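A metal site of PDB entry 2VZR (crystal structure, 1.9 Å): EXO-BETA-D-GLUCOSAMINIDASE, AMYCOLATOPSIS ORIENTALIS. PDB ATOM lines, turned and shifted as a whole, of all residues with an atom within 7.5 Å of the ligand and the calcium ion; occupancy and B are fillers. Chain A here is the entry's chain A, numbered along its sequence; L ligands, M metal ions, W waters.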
ATOM      1  N   GLN A  15      -1.026 -21.841 -19.797  1.00  0.00           N
ATOM      2  CA  GLN A  15      -0.336 -20.712 -19.152  1.00  0.00           C
ATOM      3  C   GLN A  15      -1.185 -20.053 -18.063  1.00  0.00           C
ATOM      4  O   GLN A  15      -1.577 -18.894 -18.178  1.00  0.00           O
ATOM      5  CB  GLN A  15       0.103 -19.692 -20.182  1.00  0.00           C
ATOM      6  CG  GLN A  15       0.924 -20.281 -21.324  1.00  0.00           C
ATOM      7  CD  GLN A  15       1.516 -19.204 -22.186  1.00  0.00           C
ATOM      8  OE1 GLN A  15       2.415 -18.487 -21.764  1.00  0.00           O
ATOM      9  NE2 GLN A  15       1.003 -19.072 -23.399  1.00  0.00           N
ATOM     10  N   GLY A  16      -1.470 -20.834 -17.026  1.00  0.00           N
ATOM     11  CA  GLY A  16      -2.234 -20.370 -15.879  1.00  0.00           C
ATOM     12  C   GLY A  16      -1.984 -21.300 -14.706  1.00  0.00           C
ATOM     13  O   GLY A  16      -1.274 -22.307 -14.835  1.00  0.00           O
ATOM     14  N   GLU A  19      -5.248 -21.318  -8.127  1.00  0.00           N
ATOM     15  CA  GLU A  19      -4.898 -20.609  -6.903  1.00  0.00           C
ATOM     16  C   GLU A  19      -6.144 -20.431  -6.069  1.00  0.00           C
ATOM     17  O   GLU A  19      -7.254 -20.713  -6.524  1.00  0.00           O
ATOM     18  CB  GLU A  19      -4.187 -19.284  -7.229  1.00  0.00           C
ATOM     19  CG  GLU A  19      -2.922 -19.548  -8.069  1.00  0.00           C
ATOM     20  CD  GLU A  19      -2.046 -18.350  -8.306  1.00  0.00           C
ATOM     21  OE1 GLU A  19      -2.501 -17.204  -8.159  1.00  0.00           O
ATOM     22  OE2 GLU A  19      -0.870 -18.593  -8.669  1.00  0.00           O
ATOM     23  N   ASN A  21      -6.009 -17.912  -3.123  1.00  0.00           N
ATOM     24  CA  ASN A  21      -5.552 -16.915  -2.140  1.00  0.00           C
ATOM     25  C   ASN A  21      -6.420 -15.655  -2.040  1.00  0.00           C
ATOM     26  O   ASN A  21      -6.114 -14.747  -1.273  1.00  0.00           O
ATOM     27  CB  ASN A  21      -4.086 -16.546  -2.386  1.00  0.00           C
ATOM     28  CG  ASN A  21      -3.871 -15.836  -3.723  1.00  0.00           C
ATOM     29  OD1 ASN A  21      -4.491 -16.184  -4.723  1.00  0.00           O
ATOM     30  ND2 ASN A  21      -2.983 -14.841  -3.737  1.00  0.00           N
ATOM     31  N   HIS A  22      -7.484 -15.595  -2.828  1.00  0.00           N
ATOM     32  CA  HIS A  22      -8.441 -14.509  -2.737  1.00  0.00           C
ATOM     33  C   HIS A  22      -9.771 -15.151  -2.422  1.00  0.00           C
ATOM     34  O   HIS A  22     -10.133 -16.125  -3.073  1.00  0.00           O
ATOM     35  CB  HIS A  22      -8.526 -13.742  -4.065  1.00  0.00           C
ATOM     36  CG  HIS A  22      -7.245 -13.054  -4.441  1.00  0.00           C
ATOM     37  ND1 HIS A  22      -6.672 -12.077  -3.659  1.00  0.00           N
ATOM     38  CD2 HIS A  22      -6.449 -13.200  -5.520  1.00  0.00           C
ATOM     39  CE1 HIS A  22      -5.567 -11.654  -4.243  1.00  0.00           C
ATOM     40  NE2 HIS A  22      -5.402 -12.318  -5.372  1.00  0.00           N
ATOM     41  N   PHE A  30      -9.658 -21.124  -8.164  1.00  0.00           N
ATOM     42  CA  PHE A  30      -9.924 -20.363  -9.411  1.00  0.00           C
ATOM     43  C   PHE A  30      -8.701 -20.480 -10.309  1.00  0.00           C
ATOM     44  O   PHE A  30      -7.651 -20.944  -9.859  1.00  0.00           O
ATOM     45  CB  PHE A  30     -10.265 -18.880  -9.132  1.00  0.00           C
ATOM     46  CG  PHE A  30      -9.257 -18.167  -8.261  1.00  0.00           C
ATOM     47  CD1 PHE A  30      -8.150 -17.509  -8.816  1.00  0.00           C
ATOM     48  CD2 PHE A  30      -9.426 -18.131  -6.875  1.00  0.00           C
ATOM     49  CE1 PHE A  30      -7.217 -16.860  -8.016  1.00  0.00           C
ATOM     50  CE2 PHE A  30      -8.499 -17.479  -6.041  1.00  0.00           C
ATOM     51  CZ  PHE A  30      -7.396 -16.850  -6.612  1.00  0.00           C
ATOM     52  N   VAL A  31      -8.848 -20.051 -11.561  1.00  0.00           N
ATOM     53  CA  VAL A  31      -7.702 -19.934 -12.448  1.00  0.00           C
ATOM     54  C   VAL A  31      -7.163 -18.505 -12.502  1.00  0.00           C
ATOM     55  O   VAL A  31      -7.863 -17.554 -12.800  1.00  0.00           O
ATOM     56  CB  VAL A  31      -7.967 -20.473 -13.887  1.00  0.00           C
ATOM     57  CG1 VAL A  31      -6.730 -20.263 -14.762  1.00  0.00           C
ATOM     58  CG2 VAL A  31      -8.273 -21.942 -13.825  1.00  0.00           C
ATOM     59  N   ASN A  32      -5.887 -18.389 -12.148  1.00  0.00           N
ATOM     60  CA  ASN A  32      -5.107 -17.188 -12.396  1.00  0.00           C
ATOM     61  C   ASN A  32      -4.419 -17.337 -13.753  1.00  0.00           C
ATOM     62  O   ASN A  32      -3.520 -18.161 -13.910  1.00  0.00           O
ATOM     63  CB  ASN A  32      -4.068 -17.033 -11.287  1.00  0.00           C
ATOM     64  CG  ASN A  32      -3.210 -15.782 -11.450  1.00  0.00           C
ATOM     65  OD1 ASN A  32      -3.321 -15.062 -12.443  1.00  0.00           O
ATOM     66  ND2 ASN A  32      -2.366 -15.509 -10.463  1.00  0.00           N
ATOM     67  N   TYR A  33      -4.857 -16.567 -14.742  1.00  0.00           N
ATOM     68  CA  TYR A  33      -4.205 -16.587 -16.059  1.00  0.00           C
ATOM     69  C   TYR A  33      -2.781 -16.025 -15.932  1.00  0.00           C
ATOM     70  O   TYR A  33      -2.587 -15.006 -15.278  1.00  0.00           O
ATOM     71  CB  TYR A  33      -4.970 -15.709 -17.056  1.00  0.00           C
ATOM     72  CG  TYR A  33      -6.218 -16.266 -17.707  1.00  0.00           C
ATOM     73  CD1 TYR A  33      -7.272 -16.772 -16.941  1.00  0.00           C
ATOM     74  CD2 TYR A  33      -6.378 -16.237 -19.103  1.00  0.00           C
ATOM     75  CE1 TYR A  33      -8.424 -17.249 -17.536  1.00  0.00           C
ATOM     76  CE2 TYR A  33      -7.548 -16.724 -19.706  1.00  0.00           C
ATOM     77  CZ  TYR A  33      -8.564 -17.224 -18.911  1.00  0.00           C
ATOM     78  OH  TYR A  33      -9.717 -17.714 -19.476  1.00  0.00           O
ATOM     79  N   ASP A  34      -1.782 -16.625 -16.571  1.00  0.00           N
ATOM     80  CA  ASP A  34      -0.477 -15.946 -16.624  1.00  0.00           C
ATOM     81  C   ASP A  34      -0.639 -14.596 -17.336  1.00  0.00           C
ATOM     82  O   ASP A  34      -1.508 -14.460 -18.193  1.00  0.00           O
ATOM     83  CB  ASP A  34       0.573 -16.804 -17.311  1.00  0.00           C
ATOM     84  CG  ASP A  34       0.955 -18.010 -16.511  1.00  0.00           C
ATOM     85  OD1 ASP A  34       0.551 -18.143 -15.324  1.00  0.00           O
ATOM     86  OD2 ASP A  34       1.686 -18.843 -17.090  1.00  0.00           O
ATOM     87  N   ASN A  35       0.162 -13.593 -16.960  1.00  0.00           N
ATOM     88  CA  ASN A  35       0.027 -12.265 -17.554  1.00  0.00           C
ATOM     89  C   ASN A  35       0.794 -12.191 -18.878  1.00  0.00           C
ATOM     90  O   ASN A  35       1.835 -11.549 -18.984  1.00  0.00           O
ATOM     91  CB  ASN A  35       0.453 -11.151 -16.588  1.00  0.00           C
ATOM     92  CG  ASN A  35      -0.504 -10.979 -15.426  1.00  0.00           C
ATOM     93  OD1 ASN A  35      -0.910  -9.864 -15.085  1.00  0.00           O
ATOM     94  ND2 ASN A  35      -0.879 -12.091 -14.812  1.00  0.00           N
ATOM     95  N   VAL A  36       0.248 -12.908 -19.858  1.00  0.00           N
ATOM     96  CA  VAL A  36       0.752 -12.951 -21.233  1.00  0.00           C
ATOM     97  C   VAL A  36      -0.474 -13.073 -22.131  1.00  0.00           C
ATOM     98  O   VAL A  36      -1.523 -13.564 -21.701  1.00  0.00           O
ATOM     99  CB  VAL A  36       1.653 -14.199 -21.488  1.00  0.00           C
ATOM    100  CG1 VAL A  36       2.986 -14.071 -20.779  1.00  0.00           C
ATOM    101  CG2 VAL A  36       0.942 -15.503 -21.053  1.00  0.00           C
ATOM    102  N   SER A  39      -2.785 -16.973 -22.735  1.00  0.00           N
ATOM    103  CA  SER A  39      -3.264 -17.749 -21.602  1.00  0.00           C
ATOM    104  C   SER A  39      -4.751 -18.079 -21.810  1.00  0.00           C
ATOM    105  O   SER A  39      -5.509 -17.241 -22.308  1.00  0.00           O
ATOM    106  CB  SER A  39      -3.020 -17.000 -20.288  1.00  0.00           C
ATOM    107  OG  SER A  39      -3.355 -15.635 -20.384  1.00  0.00           O
ATOM    108  N   ALA A  60     -12.740 -11.969 -11.647  1.00  0.00           N
ATOM    109  CA  ALA A  60     -12.311 -10.809 -10.897  1.00  0.00           C
ATOM    110  C   ALA A  60     -11.146 -10.140 -11.625  1.00  0.00           C
ATOM    111  O   ALA A  60     -10.354 -10.804 -12.299  1.00  0.00           O
ATOM    112  CB  ALA A  60     -11.899 -11.217  -9.460  1.00  0.00           C
ATOM    113  N   ASN A  61     -11.060  -8.820 -11.456  1.00  0.00           N
ATOM    114  CA  ASN A  61      -9.999  -7.983 -12.049  1.00  0.00           C
ATOM    115  C   ASN A  61      -9.685  -6.798 -11.121  1.00  0.00           C
ATOM    116  O   ASN A  61     -10.329  -5.752 -11.167  1.00  0.00           O
ATOM    117  CB  ASN A  61     -10.413  -7.523 -13.473  1.00  0.00           C
ATOM    118  CG  ASN A  61      -9.382  -6.624 -14.142  1.00  0.00           C
ATOM    119  OD1 ASN A  61      -8.290  -6.369 -13.611  1.00  0.00           O
ATOM    120  ND2 ASN A  61      -9.717  -6.135 -15.344  1.00  0.00           N
ATOM    121  N   GLY A  62      -8.701  -7.007 -10.243  1.00  0.00           N
ATOM    122  CA  GLY A  62      -8.283  -5.994  -9.280  1.00  0.00           C
ATOM    123  C   GLY A  62      -7.273  -5.018  -9.848  1.00  0.00           C
ATOM    124  O   GLY A  62      -6.260  -4.722  -9.217  1.00  0.00           O
ATOM    125  N   THR A  63      -7.547  -4.547 -11.079  1.00  0.00           N
ATOM    126  CA  THR A  63      -6.777  -3.491 -11.743  1.00  0.00           C
ATOM    127  C   THR A  63      -7.732  -2.549 -12.479  1.00  0.00           C
ATOM    128  O   THR A  63      -8.912  -2.861 -12.631  1.00  0.00           O
ATOM    129  CB  THR A  63      -5.753  -4.039 -12.773  1.00  0.00           C
ATOM    130  OG1 THR A  63      -6.441  -4.432 -13.986  1.00  0.00           O
ATOM    131  CG2 THR A  63      -4.923  -5.192 -12.196  1.00  0.00           C
ATOM    132  N   ARG A  67      -9.333  -6.566 -19.225  1.00  0.00           N
ATOM    133  CA  ARG A  67      -8.594  -7.717 -19.688  1.00  0.00           C
ATOM    134  C   ARG A  67      -9.481  -8.568 -20.607  1.00  0.00           C
ATOM    135  O   ARG A  67     -10.234  -9.427 -20.148  1.00  0.00           O
ATOM    136  CB  ARG A  67      -8.080  -8.511 -18.502  1.00  0.00           C
ATOM    137  CG  ARG A  67      -7.059  -7.703 -17.709  1.00  0.00           C
ATOM    138  CD  ARG A  67      -6.284  -8.598 -16.850  1.00  0.00           C
ATOM    139  NE  ARG A  67      -5.286  -7.893 -16.045  1.00  0.00           N
ATOM    140  CZ  ARG A  67      -4.608  -8.485 -15.068  1.00  0.00           C
ATOM    141  NH1 ARG A  67      -4.856  -9.757 -14.763  1.00  0.00           N
ATOM    142  NH2 ARG A  67      -3.697  -7.807 -14.381  1.00  0.00           N
ATOM    143  N   TRP A  90      -9.507  -8.151  -5.997  1.00  0.00           N
ATOM    144  CA  TRP A  90      -9.495  -9.529  -6.478  1.00  0.00           C
ATOM    145  C   TRP A  90     -10.570 -10.440  -5.845  1.00  0.00           C
ATOM    146  O   TRP A  90     -11.082 -11.311  -6.539  1.00  0.00           O
ATOM    147  CB  TRP A  90      -8.094 -10.112  -6.374  1.00  0.00           C
ATOM    148  CG  TRP A  90      -7.080  -9.396  -7.233  1.00  0.00           C
ATOM    149  CD1 TRP A  90      -6.127  -8.510  -6.801  1.00  0.00           C
ATOM    150  CD2 TRP A  90      -6.943  -9.483  -8.655  1.00  0.00           C
ATOM    151  NE1 TRP A  90      -5.383  -8.063  -7.874  1.00  0.00           N
ATOM    152  CE2 TRP A  90      -5.870  -8.622  -9.018  1.00  0.00           C
ATOM    153  CE3 TRP A  90      -7.614 -10.191  -9.663  1.00  0.00           C
ATOM    154  CZ2 TRP A  90      -5.459  -8.462 -10.354  1.00  0.00           C
ATOM    155  CZ3 TRP A  90      -7.194 -10.040 -10.996  1.00  0.00           C
ATOM    156  CH2 TRP A  90      -6.130  -9.190 -11.324  1.00  0.00           C
ATOM    157  N   ASN A 117      -1.601  -8.402 -20.685  1.00  0.00           N
ATOM    158  CA  ASN A 117      -1.985  -8.492 -19.264  1.00  0.00           C
ATOM    159  C   ASN A 117      -2.650  -9.803 -18.873  1.00  0.00           C
ATOM    160  O   ASN A 117      -2.952 -10.023 -17.707  1.00  0.00           O
ATOM    161  CB  ASN A 117      -2.878  -7.304 -18.884  1.00  0.00           C
ATOM    162  CG  ASN A 117      -2.101  -6.005 -18.836  1.00  0.00           C
ATOM    163  OD1 ASN A 117      -1.035  -5.930 -18.226  1.00  0.00           O
ATOM    164  ND2 ASN A 117      -2.628  -4.972 -19.473  1.00  0.00           N
ATOM    165  N   GLY A 118      -2.859 -10.676 -19.868  1.00  0.00           N
ATOM    166  CA  GLY A 118      -3.523 -11.944 -19.623  1.00  0.00           C
ATOM    167  C   GLY A 118      -5.007 -11.770 -19.311  1.00  0.00           C
ATOM    168  O   GLY A 118      -5.604 -10.754 -19.676  1.00  0.00           O
ATOM    169  N   GLY A 119      -5.588 -12.758 -18.651  1.00  0.00           N
ATOM    170  CA  GLY A 119      -7.005 -12.749 -18.364  1.00  0.00           C
ATOM    171  C   GLY A 119      -7.322 -12.256 -16.967  1.00  0.00           C
ATOM    172  O   GLY A 119      -6.418 -12.095 -16.123  1.00  0.00           O
ATOM    173  N   PRO A 120      -8.619 -12.016 -16.689  1.00  0.00           N
ATOM    174  CA  PRO A 120      -9.048 -11.811 -15.329  1.00  0.00           C
ATOM    175  C   PRO A 120      -8.808 -13.146 -14.629  1.00  0.00           C
ATOM    176  O   PRO A 120      -8.555 -14.145 -15.320  1.00  0.00           O
ATOM    177  CB  PRO A 120     -10.553 -11.540 -15.484  1.00  0.00           C
ATOM    178  CG  PRO A 120     -10.937 -12.249 -16.732  1.00  0.00           C
ATOM    179  CD  PRO A 120      -9.752 -12.049 -17.639  1.00  0.00           C
ATOM    180  N   ASN A 121      -8.847 -13.177 -13.290  1.00  0.00           N
ATOM    181  CA  ASN A 121      -8.929 -14.448 -12.586  1.00  0.00           C
ATOM    182  C   ASN A 121     -10.337 -14.957 -12.881  1.00  0.00           C
ATOM    183  O   ASN A 121     -11.290 -14.172 -12.888  1.00  0.00           O
ATOM    184  CB  ASN A 121      -8.757 -14.269 -11.074  1.00  0.00           C
ATOM    185  CG  ASN A 121      -7.322 -13.935 -10.662  1.00  0.00           C
ATOM    186  OD1 ASN A 121      -6.393 -14.028 -11.472  1.00  0.00           O
ATOM    187  ND2 ASN A 121      -7.149 -13.557  -9.394  1.00  0.00           N
HETATM  188  C1  LIG L   1      -2.097 -10.190  -8.397  1.00  0.00           C
HETATM  189  C2  LIG L   1      -3.267 -11.071  -7.936  1.00  0.00           C
HETATM  190  C3  LIG L   1      -3.456 -12.233  -8.904  1.00  0.00           C
HETATM  191  C4  LIG L   1      -3.683 -11.688 -10.299  1.00  0.00           C
HETATM  192  C5  LIG L   1      -2.501 -10.809 -10.734  1.00  0.00           C
HETATM  193  C6  LIG L   1      -2.749 -10.177 -12.106  1.00  0.00           C
HETATM  194  O1  LIG L   1      -0.895 -10.924  -8.258  1.00  0.00           O
HETATM  195  O2  LIG L   1      -3.056 -11.573  -6.625  1.00  0.00           O
HETATM  196  O3  LIG L   1      -4.562 -13.025  -8.506  1.00  0.00           O
HETATM  197  O4  LIG L   1      -3.901 -12.765 -11.186  1.00  0.00           O
HETATM  198  O5  LIG L   1      -2.267  -9.783  -9.757  1.00  0.00           O
HETATM  199  O6  LIG L   1      -3.107 -10.878 -13.085  1.00  0.00           O
HETATM  200  O7  LIG L   1      -2.618  -8.935 -12.204  1.00  0.00           O
HETATM  201 CA    CA M   1      -2.622 -13.276 -13.730  1.00  0.00          CA
HETATM  202  O   HOH W   1      -5.479 -13.622 -13.876  1.00  0.00           O
HETATM  203  O   HOH W   2      -1.189 -13.467  -6.037  1.00  0.00           O
HETATM  204  O   HOH W   3       0.072 -13.614  -9.615  1.00  0.00           O
HETATM  205  O   HOH W   4      -4.112 -15.464  -7.192  1.00  0.00           O
HETATM  206  O   HOH W   5       1.159  -9.299  -7.767  1.00  0.00           O
HETATM  207  O   HOH W   6      -2.917  -9.385  -4.604  1.00  0.00           O
HETATM  208  O   HOH W   7      -3.584 -12.167 -15.961  1.00  0.00           O
HETATM  209  O   HOH W   8      -1.933  -6.897 -10.387  1.00  0.00           O
HETATM  210  O   HOH W   9      -0.725 -13.667 -12.695  1.00  0.00           O
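An oxygen (O3) of the ligand sits at hydrogen-bond distance from the side-chain amide nitrogen (ND2) of Asn 121, at 2.8 Å. A ring nitrogen (NE2) of His 22 sits at hydrogen-bond distance from an oxygen (O2) of the ligand, at 2.8 Å. The guanidinium group of Arg 67 is in salt-bridge range of an oxygen (O7) of the ligand (2.7 Å).
The backbone NH (N) of Ala 60 is in hydrogen-bond range of the backbone carbonyl oxygen (O) of Asn 121. The side-chain amide oxygen (OD1) of Asn 121 sits close to the side-chain amide oxygen (OD1) of Asn 32 (3.4 Å). ND2 of Asn 32 sits at hydrogen-bond distance from OE1 of Glu 19 (2.9 Å). The guanidinium group of Arg 67 sits at hydrogen-bond distance from the backbone carbonyl oxygen of Gly 119 (3.1 Å). OD1 of Asn 35 lies close to O of Asn 117, at 3.3 Å.
CZ2 of Trp 90 touches O7 of the ligand, 3.4 Å away. Hydrophobic or aromatic side chains that line the ligand: His 22 and Trp 90. Six residues have an atom within 4 Å of the ligand: His 22, Asn 32, Asn 35, Arg 67, Trp 90 and Asn 121.
The calcium ion is bound by water W9 (2.2 Å). The calcium ion is bound by OD1 of Asn 32 (2.3 Å). O of Tyr 33 binds the calcium ion (2.3 Å). ND2 of Asn 35 binds the calcium ion, at 2.4 Å. An oxygen (O6) of the ligand binds the calcium ion. The calcium ion is bound by water W7 (2.7 Å). Water W1 is bound to the calcium ion. The calcium ion is bound by O4 of the ligand, at 2.9 Å. The calcium ion has eight donor atoms within binding distance.
Water W7 lies within hydrogen-bond range of O of Asn 117 (2.8 Å), O of Gly 119 (2.8 Å) and NH1 of Arg 67 (3.0 Å). Water W2 bridges an oxygen (O2) of the ligand (2.7 Å) and the side-chain amide nitrogen of Asn 21 (3.2 Å). Water W4 lies within hydrogen-bond range of OE1 of Glu 19, OD1 of Asn 21 and O3 of the ligand. Water W3 bridges an oxygen (O1) of the ligand (3.2 Å) and the side-chain amide nitrogen of Asn 32 (3.2 Å).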
